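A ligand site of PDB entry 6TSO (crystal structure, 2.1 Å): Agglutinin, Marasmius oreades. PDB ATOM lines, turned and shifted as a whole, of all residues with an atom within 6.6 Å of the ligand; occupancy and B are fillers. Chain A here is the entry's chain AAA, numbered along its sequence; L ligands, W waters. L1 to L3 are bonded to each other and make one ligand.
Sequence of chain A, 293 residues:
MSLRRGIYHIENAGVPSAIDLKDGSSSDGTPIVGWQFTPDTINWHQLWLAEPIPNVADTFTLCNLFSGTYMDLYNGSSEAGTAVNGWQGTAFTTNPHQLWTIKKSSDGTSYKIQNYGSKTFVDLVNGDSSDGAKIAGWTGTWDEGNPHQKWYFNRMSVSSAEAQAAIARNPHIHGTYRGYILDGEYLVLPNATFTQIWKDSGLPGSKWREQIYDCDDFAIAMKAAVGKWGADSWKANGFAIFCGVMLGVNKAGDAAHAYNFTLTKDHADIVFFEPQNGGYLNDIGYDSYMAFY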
ATOM      1  N   HIS A   9      -1.812  21.576   6.960  1.00  0.00           N
ATOM      2  CA  HIS A   9      -1.005  21.633   8.204  1.00  0.00           C
ATOM      3  C   HIS A   9      -1.082  23.087   8.649  1.00  0.00           C
ATOM      4  O   HIS A   9      -0.595  23.958   7.887  1.00  0.00           O
ATOM      5  CB  HIS A   9       0.389  21.065   7.943  1.00  0.00           C
ATOM      6  CG  HIS A   9       1.186  20.835   9.168  1.00  0.00           C
ATOM      7  ND1 HIS A   9       2.314  21.573   9.452  1.00  0.00           N
ATOM      8  CD2 HIS A   9       1.003  19.981  10.212  1.00  0.00           C
ATOM      9  CE1 HIS A   9       2.808  21.170  10.611  1.00  0.00           C
ATOM     10  NE2 HIS A   9       2.001  20.196  11.106  1.00  0.00           N
ATOM     11  N   ASP A  20      -2.888  20.816  16.709  1.00  0.00           N
ATOM     12  CA  ASP A  20      -2.624  19.401  17.003  1.00  0.00           C
ATOM     13  C   ASP A  20      -3.770  18.919  17.893  1.00  0.00           C
ATOM     14  O   ASP A  20      -4.048  19.544  18.910  1.00  0.00           O
ATOM     15  CB  ASP A  20      -1.220  19.260  17.608  1.00  0.00           C
ATOM     16  CG  ASP A  20      -0.809  17.857  18.005  1.00  0.00           C
ATOM     17  OD1 ASP A  20      -1.492  17.244  18.885  1.00  0.00           O
ATOM     18  OD2 ASP A  20       0.201  17.385  17.462  1.00  0.00           O
ATOM     19  N   LEU A  21      -4.456  17.864  17.499  1.00  0.00           N
ATOM     20  CA  LEU A  21      -5.475  17.231  18.347  1.00  0.00           C
ATOM     21  C   LEU A  21      -4.722  16.260  19.237  1.00  0.00           C
ATOM     22  O   LEU A  21      -4.107  15.315  18.726  1.00  0.00           O
ATOM     23  CB  LEU A  21      -6.494  16.559  17.436  1.00  0.00           C
ATOM     24  CG  LEU A  21      -7.544  15.737  18.150  1.00  0.00           C
ATOM     25  CD1 LEU A  21      -8.489  16.623  18.957  1.00  0.00           C
ATOM     26  CD2 LEU A  21      -8.327  14.914  17.137  1.00  0.00           C
ATOM     27  N   LYS A  22      -4.711  16.526  20.539  1.00  0.00           N
ATOM     28  CA  LYS A  22      -3.728  15.890  21.462  1.00  0.00           C
ATOM     29  C   LYS A  22      -3.883  14.355  21.371  1.00  0.00           C
ATOM     30  O   LYS A  22      -4.998  13.860  21.536  1.00  0.00           O
ATOM     31  CB  LYS A  22      -3.945  16.441  22.867  1.00  0.00           C
ATOM     32  CG  LYS A  22      -2.668  16.378  23.685  1.00  0.00           C
ATOM     33  CD  LYS A  22      -2.745  16.983  25.044  1.00  0.00           C
ATOM     34  CE  LYS A  22      -1.530  16.567  25.840  1.00  0.00           C
ATOM     35  NZ  LYS A  22      -1.591  17.076  27.223  1.00  0.00           N
ATOM     36  N   ASP A  23      -2.791  13.654  21.102  1.00  0.00           N
ATOM     37  CA  ASP A  23      -2.693  12.159  21.002  1.00  0.00           C
ATOM     38  C   ASP A  23      -3.604  11.655  19.881  1.00  0.00           C
ATOM     39  O   ASP A  23      -3.816  10.438  19.783  1.00  0.00           O
ATOM     40  CB  ASP A  23      -3.015  11.466  22.330  1.00  0.00           C
ATOM     41  CG  ASP A  23      -2.402  10.076  22.479  1.00  0.00           C
ATOM     42  OD1 ASP A  23      -1.212   9.904  22.135  1.00  0.00           O
ATOM     43  OD2 ASP A  23      -3.124   9.150  22.924  1.00  0.00           O
ATOM     44  N   GLY A  24      -4.079  12.519  18.986  1.00  0.00           N
ATOM     45  CA  GLY A  24      -4.960  12.124  17.884  1.00  0.00           C
ATOM     46  C   GLY A  24      -6.247  11.482  18.390  1.00  0.00           C
ATOM     47  O   GLY A  24      -6.905  10.777  17.579  1.00  0.00           O
ATOM     48  N   VAL A  33      -4.287  21.696  20.669  1.00  0.00           N
ATOM     49  CA  VAL A  33      -3.185  22.449  21.328  1.00  0.00           C
ATOM     50  C   VAL A  33      -2.136  22.786  20.273  1.00  0.00           C
ATOM     51  O   VAL A  33      -2.139  22.166  19.191  1.00  0.00           O
ATOM     52  CB  VAL A  33      -2.586  21.627  22.487  1.00  0.00           C
ATOM     53  CG1 VAL A  33      -3.635  21.289  23.542  1.00  0.00           C
ATOM     54  CG2 VAL A  33      -1.910  20.349  22.008  1.00  0.00           C
ATOM     55  N   TRP A  35       1.685  22.348  19.064  1.00  0.00           N
ATOM     56  CA  TRP A  35       2.723  21.310  19.154  1.00  0.00           C
ATOM     57  C   TRP A  35       3.729  21.540  18.037  1.00  0.00           C
ATOM     58  O   TRP A  35       3.308  21.983  16.965  1.00  0.00           O
ATOM     59  CB  TRP A  35       2.099  19.897  19.095  1.00  0.00           C
ATOM     60  CG  TRP A  35       2.852  18.872  19.862  1.00  0.00           C
ATOM     61  CD1 TRP A  35       4.009  18.236  19.498  1.00  0.00           C
ATOM     62  CD2 TRP A  35       2.520  18.370  21.182  1.00  0.00           C
ATOM     63  NE1 TRP A  35       4.383  17.331  20.461  1.00  0.00           N
ATOM     64  CE2 TRP A  35       3.516  17.426  21.520  1.00  0.00           C
ATOM     65  CE3 TRP A  35       1.461  18.581  22.068  1.00  0.00           C
ATOM     66  CZ2 TRP A  35       3.499  16.740  22.739  1.00  0.00           C
ATOM     67  CZ3 TRP A  35       1.444  17.886  23.257  1.00  0.00           C
ATOM     68  CH2 TRP A  35       2.435  16.956  23.570  1.00  0.00           C
ATOM     69  N   GLN A  36       5.003  21.268  18.283  1.00  0.00           N
ATOM     70  CA  GLN A  36       6.065  21.392  17.257  1.00  0.00           C
ATOM     71  C   GLN A  36       5.836  20.296  16.215  1.00  0.00           C
ATOM     72  O   GLN A  36       5.067  19.369  16.459  1.00  0.00           O
ATOM     73  CB  GLN A  36       7.469  21.286  17.883  1.00  0.00           C
ATOM     74  CG  GLN A  36       7.737  19.959  18.551  1.00  0.00           C
ATOM     75  CD  GLN A  36       9.103  19.953  19.183  1.00  0.00           C
ATOM     76  OE1 GLN A  36      10.104  20.168  18.489  1.00  0.00           O
ATOM     77  NE2 GLN A  36       9.132  19.797  20.513  1.00  0.00           N
ATOM     78  N   PHE A  37       6.506  20.398  15.076  1.00  0.00           N
ATOM     79  CA  PHE A  37       6.285  19.495  13.942  1.00  0.00           C
ATOM     80  C   PHE A  37       7.598  19.292  13.204  1.00  0.00           C
ATOM     81  O   PHE A  37       8.564  20.010  13.476  1.00  0.00           O
ATOM     82  CB  PHE A  37       5.191  20.135  13.070  1.00  0.00           C
ATOM     83  CG  PHE A  37       5.505  21.522  12.611  1.00  0.00           C
ATOM     84  CD1 PHE A  37       6.138  21.738  11.403  1.00  0.00           C
ATOM     85  CD2 PHE A  37       5.017  22.613  13.316  1.00  0.00           C
ATOM     86  CE1 PHE A  37       6.369  23.027  10.955  1.00  0.00           C
ATOM     87  CE2 PHE A  37       5.224  23.906  12.851  1.00  0.00           C
ATOM     88  CZ  PHE A  37       5.918  24.108  11.682  1.00  0.00           C
ATOM     89  N   THR A  38       7.627  18.302  12.316  1.00  0.00           N
ATOM     90  CA  THR A  38       8.819  18.002  11.492  1.00  0.00           C
ATOM     91  C   THR A  38       8.355  18.205  10.050  1.00  0.00           C
ATOM     92  O   THR A  38       7.407  17.570   9.622  1.00  0.00           O
ATOM     93  CB  THR A  38       9.388  16.611  11.779  1.00  0.00           C
ATOM     94  OG1 THR A  38       9.404  16.353  13.182  1.00  0.00           O
ATOM     95  CG2 THR A  38      10.808  16.438  11.290  1.00  0.00           C
ATOM     96  N   PRO A  39       9.001  19.105   9.281  1.00  0.00           N
ATOM     97  CA  PRO A  39       8.721  19.240   7.854  1.00  0.00           C
ATOM     98  C   PRO A  39       8.954  17.925   7.091  1.00  0.00           C
ATOM     99  O   PRO A  39       9.765  17.157   7.545  1.00  0.00           O
ATOM    100  CB  PRO A  39       9.735  20.286   7.355  1.00  0.00           C
ATOM    101  CG  PRO A  39      10.180  21.006   8.618  1.00  0.00           C
ATOM    102  CD  PRO A  39      10.096  19.969   9.724  1.00  0.00           C
ATOM    103  N   THR A  41       7.377  15.256   6.746  1.00  0.00           N
ATOM    104  CA  THR A  41       6.848  14.048   7.399  1.00  0.00           C
ATOM    105  C   THR A  41       5.325  14.102   7.331  1.00  0.00           C
ATOM    106  O   THR A  41       4.748  15.161   6.976  1.00  0.00           O
ATOM    107  CB  THR A  41       7.271  13.877   8.868  1.00  0.00           C
ATOM    108  OG1 THR A  41       6.748  14.949   9.675  1.00  0.00           O
ATOM    109  CG2 THR A  41       8.784  13.828   9.046  1.00  0.00           C
ATOM    110  N   ILE A  42       4.704  12.976   7.664  1.00  0.00           N
ATOM    111  CA  ILE A  42       3.282  12.902   8.073  1.00  0.00           C
ATOM    112  C   ILE A  42       3.232  13.336   9.529  1.00  0.00           C
ATOM    113  O   ILE A  42       3.820  12.617  10.351  1.00  0.00           O
ATOM    114  CB  ILE A  42       2.731  11.476   7.839  1.00  0.00           C
ATOM    115  CG1 ILE A  42       2.738  11.133   6.339  1.00  0.00           C
ATOM    116  CG2 ILE A  42       1.363  11.308   8.475  1.00  0.00           C
ATOM    117  CD1 ILE A  42       2.131  12.207   5.440  1.00  0.00           C
ATOM    118  N   ASN A  43       2.690  14.535   9.817  1.00  0.00           N
ATOM    119  CA  ASN A  43       2.437  15.001  11.206  1.00  0.00           C
ATOM    120  C   ASN A  43       1.042  14.464  11.583  1.00  0.00           C
ATOM    121  O   ASN A  43       0.033  15.112  11.292  1.00  0.00           O
ATOM    122  CB  ASN A  43       2.613  16.515  11.304  1.00  0.00           C
ATOM    123  CG  ASN A  43       4.070  16.881  11.143  1.00  0.00           C
ATOM    124  OD1 ASN A  43       4.849  16.587  12.045  1.00  0.00           O
ATOM    125  ND2 ASN A  43       4.431  17.495  10.020  1.00  0.00           N
ATOM    126  N   TRP A  44       1.050  13.247  12.102  1.00  0.00           N
ATOM    127  CA  TRP A  44      -0.125  12.345  12.239  1.00  0.00           C
ATOM    128  C   TRP A  44      -1.327  13.008  12.943  1.00  0.00           C
ATOM    129  O   TRP A  44      -2.485  12.639  12.580  1.00  0.00           O
ATOM    130  CB  TRP A  44       0.291  11.084  12.994  1.00  0.00           C
ATOM    131  CG  TRP A  44       0.953  10.094  12.086  1.00  0.00           C
ATOM    132  CD1 TRP A  44       2.287   9.894  11.927  1.00  0.00           C
ATOM    133  CD2 TRP A  44       0.295   9.251  11.115  1.00  0.00           C
ATOM    134  NE1 TRP A  44       2.499   8.949  10.967  1.00  0.00           N
ATOM    135  CE2 TRP A  44       1.303   8.540  10.451  1.00  0.00           C
ATOM    136  CE3 TRP A  44      -1.041   9.008  10.805  1.00  0.00           C
ATOM    137  CZ2 TRP A  44       1.018   7.586   9.478  1.00  0.00           C
ATOM    138  CZ3 TRP A  44      -1.324   8.076   9.831  1.00  0.00           C
ATOM    139  CH2 TRP A  44      -0.313   7.374   9.171  1.00  0.00           C
ATOM    140  N   HIS A  45      -1.104  13.902  13.908  1.00  0.00           N
ATOM    141  CA  HIS A  45      -2.245  14.493  14.675  1.00  0.00           C
ATOM    142  C   HIS A  45      -2.540  15.922  14.232  1.00  0.00           C
ATOM    143  O   HIS A  45      -3.378  16.561  14.901  1.00  0.00           O
ATOM    144  CB  HIS A  45      -1.936  14.445  16.167  1.00  0.00           C
ATOM    145  CG  HIS A  45      -1.629  13.074  16.627  1.00  0.00           C
ATOM    146  ND1 HIS A  45      -0.933  12.856  17.788  1.00  0.00           N
ATOM    147  CD2 HIS A  45      -1.938  11.858  16.119  1.00  0.00           C
ATOM    148  CE1 HIS A  45      -0.830  11.544  17.988  1.00  0.00           C
ATOM    149  NE2 HIS A  45      -1.440  10.911  16.985  1.00  0.00           N
ATOM    150  N   GLN A  46      -1.917  16.381  13.140  1.00  0.00           N
ATOM    151  CA  GLN A  46      -1.823  17.832  12.835  1.00  0.00           C
ATOM    152  C   GLN A  46      -2.349  18.106  11.400  1.00  0.00           C
ATOM    153  O   GLN A  46      -2.071  19.196  10.911  1.00  0.00           O
ATOM    154  CB  GLN A  46      -0.366  18.281  13.036  1.00  0.00           C
ATOM    155  CG  GLN A  46       0.180  18.149  14.476  1.00  0.00           C
ATOM    156  CD  GLN A  46       1.653  18.525  14.586  1.00  0.00           C
ATOM    157  OE1 GLN A  46       2.272  18.889  13.593  1.00  0.00           O
ATOM    158  NE2 GLN A  46       2.232  18.471  15.783  1.00  0.00           N
ATOM    159  N   PHE A  66      -6.783  12.144  11.015  1.00  0.00           N
ATOM    160  CA  PHE A  66      -6.504  10.972  11.872  1.00  0.00           C
ATOM    161  C   PHE A  66      -7.748  10.557  12.682  1.00  0.00           C
ATOM    162  O   PHE A  66      -8.099   9.367  12.676  1.00  0.00           O
ATOM    163  CB  PHE A  66      -5.382  11.261  12.874  1.00  0.00           C
ATOM    164  CG  PHE A  66      -4.945  10.015  13.586  1.00  0.00           C
ATOM    165  CD1 PHE A  66      -4.413   8.964  12.870  1.00  0.00           C
ATOM    166  CD2 PHE A  66      -5.113   9.884  14.949  1.00  0.00           C
ATOM    167  CE1 PHE A  66      -4.019   7.788  13.514  1.00  0.00           C
ATOM    168  CE2 PHE A  66      -4.723   8.726  15.604  1.00  0.00           C
ATOM    169  CZ  PHE A  66      -4.194   7.667  14.884  1.00  0.00           C
ATOM    170  N   ASP A 131       5.009  22.624  23.707  1.00  0.00           N
ATOM    171  CA  ASP A 131       4.221  21.446  23.267  1.00  0.00           C
ATOM    172  C   ASP A 131       3.057  21.232  24.230  1.00  0.00           C
ATOM    173  O   ASP A 131       3.345  20.941  25.392  1.00  0.00           O
ATOM    174  CB  ASP A 131       5.104  20.207  23.197  1.00  0.00           C
ATOM    175  CG  ASP A 131       6.061  20.246  22.029  1.00  0.00           C
ATOM    176  OD1 ASP A 131       5.776  20.995  21.077  1.00  0.00           O
ATOM    177  OD2 ASP A 131       7.076  19.499  22.055  1.00  0.00           O
HETATM  178  C1  LIG L   1       4.525  11.514  16.906  1.00  0.00           C
HETATM  179  C2  LIG L   1       5.791  10.671  17.080  1.00  0.00           C
HETATM  180  C3  LIG L   1       5.427   9.339  17.708  1.00  0.00           C
HETATM  181  C4  LIG L   1       4.362   8.667  16.889  1.00  0.00           C
HETATM  182  C5  LIG L   1       3.139   9.558  16.803  1.00  0.00           C
HETATM  183  C6  LIG L   1       2.030   9.024  15.918  1.00  0.00           C
HETATM  184  O1  LIG L   1       6.712  11.415  17.878  1.00  0.00           O
HETATM  185  O2  LIG L   1       6.580   8.534  17.729  1.00  0.00           O
HETATM  186  O3  LIG L   1       4.791   8.436  15.534  1.00  0.00           O
HETATM  187  O4  LIG L   1       3.499  10.797  16.204  1.00  0.00           O
HETATM  188  C1  LG2 L   2       2.376  12.415  19.712  1.00  0.00           C
HETATM  189  C2  LG2 L   2       2.963  12.754  18.327  1.00  0.00           C
HETATM  190  C3  LG2 L   2       3.361  14.224  18.234  1.00  0.00           C
HETATM  191  C4  LG2 L   2       2.164  15.063  18.697  1.00  0.00           C
HETATM  192  C5  LG2 L   2       1.660  14.618  20.086  1.00  0.00           C
HETATM  193  C6  LG2 L   2       0.411  15.397  20.468  1.00  0.00           C
HETATM  194  O1  LG2 L   2       1.807  11.163  19.555  1.00  0.00           O
HETATM  195  O2  LG2 L   2       4.064  11.863  18.135  1.00  0.00           O
HETATM  196  O3  LG2 L   2       3.785  14.665  16.895  1.00  0.00           O
HETATM  197  O4  LG2 L   2       1.119  14.972  17.696  1.00  0.00           O
HETATM  198  O5  LG2 L   2       1.311  13.256  20.123  1.00  0.00           O
HETATM  199  O6  LG2 L   2      -0.724  14.869  19.744  1.00  0.00           O
HETATM  200  C1  LG3 L   3       4.407  15.822  16.730  1.00  0.00           C
HETATM  201  C2  LG3 L   3       4.937  15.943  15.282  1.00  0.00           C
HETATM  202  C3  LG3 L   3       6.341  15.329  15.110  1.00  0.00           C
HETATM  203  C4  LG3 L   3       7.249  15.752  16.257  1.00  0.00           C
HETATM  204  C5  LG3 L   3       6.574  15.388  17.600  1.00  0.00           C
HETATM  205  C6  LG3 L   3       7.435  15.663  18.791  1.00  0.00           C
HETATM  206  O1  LG3 L   3       4.020  15.308  14.380  1.00  0.00           O
HETATM  207  O2  LG3 L   3       6.831  15.725  13.801  1.00  0.00           O
HETATM  208  O3  LG3 L   3       7.519  17.147  16.150  1.00  0.00           O
HETATM  209  O4  LG3 L   3       5.409  16.175  17.689  1.00  0.00           O
HETATM  210  O5  LG3 L   3       6.704  15.519  20.025  1.00  0.00           O
HETATM  211  O   HOH W   1       3.625  12.456  13.488  1.00  0.00           O
HETATM  212  O   HOH W   2       6.381  12.569  20.300  1.00  0.00           O
HETATM  213  O   HOH W   3       6.153  13.878  12.111  1.00  0.00           O
HETATM  214  O   HOH W   4       0.417  12.052  22.526  1.00  0.00           O
HETATM  215  O   HOH W   5       1.610  14.844  15.021  1.00  0.00           O
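O3 of LG3 L3 lies within hydrogen-bond range of O of Gln 36 (3.3 Å).
An oxygen (O4) of LG2 L2 sits at hydrogen-bond distance from the side-chain carboxylate of Asp 20.
The backbone NH (N) of Asp 23 lies within hydrogen-bond range of an oxygen (O6) of LG2 L2, at 2.8 Å.
N of Thr 38 sits at hydrogen-bond distance from O2 of LG3 L3 (3.1 Å).
The side-chain hydroxyl of Thr 38 is in hydrogen-bond range of an oxygen (O2) of LG3 L3 (2.7 Å).
An oxygen (O6) of LG2 L2 is in hydrogen-bond range of a ring nitrogen (ND1) of His 45 (2.8 Å).
O2 of LG3 L3 lies within hydrogen-bond range of OD1 of Asn 43 (2.8 Å).
The indole nitrogen of Trp 35 sits at hydrogen-bond distance from an oxygen (O5) of LG3 L3, 3.0 Å away.
The backbone NH (N) of Val 33 sits at hydrogen-bond distance from the backbone carbonyl oxygen (O) of Asp 20 (2.8 Å).
The side-chain amide nitrogen (NE2) of Gln 36 is in hydrogen-bond range of the side-chain carboxylate (OD2) of Asp 131 (2.6 Å).
The backbone carbonyl oxygen (O) of Gln 36 lies within hydrogen-bond range of the side-chain amide nitrogen (NE2) of Gln 46.
The backbone carbonyl oxygen of His 45 sits at hydrogen-bond distance from the backbone NH of Leu 21, 3.1 Å away.
OD2 of Asp 20 is in hydrogen-bond range of NE2 of Gln 46, 2.9 Å away.
ND1 of His 45 lies within hydrogen-bond range of N of Gly 24 (3.4 Å).
The side-chain amide oxygen (OE1) of Gln 46 sits at hydrogen-bond distance from a ring nitrogen (NE2) of His 9, 2.8 Å away.
The backbone carbonyl oxygen (O) of Thr 38 lies within hydrogen-bond range of the side-chain hydroxyl (OG1) of Thr 41, at 2.7 Å.
Residues that only touch the ligand: Phe 37 (3.5 Å), Gln 46 (3.6 Å), Leu 21 (3.6 Å), Lys 22 (3.6 Å) and Trp 44 (3.98 Å).
Along chain A the residues within 4 Å of the ligand span positions 20 to 46.
The nearest printed residue that does not touch the ligand is Gly 24 (4.2 Å).
Water W5 lies within hydrogen-bond range of O1 of LG3 L3, N of His 45 and N of Trp 44.
Water W3 lies within hydrogen-bond range of O2 of LG3 L3 (2.6 Å), OG1 of Thr 41 (2.7 Å), OD1 of Asn 43 (3.0 Å) and O of Ile 42 (3.2 Å).
Water W4 lies within hydrogen-bond range of OD1 of Asp 23 (2.7 Å) and O5 of LG2 L2 (2.8 Å).
Water W1 lies within hydrogen-bond range of an oxygen (O1) of LG3 L3 (3.0 Å), the backbone NH of Trp 44 (3.0 Å) and the backbone carbonyl oxygen of Ile 42 (3.1 Å).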
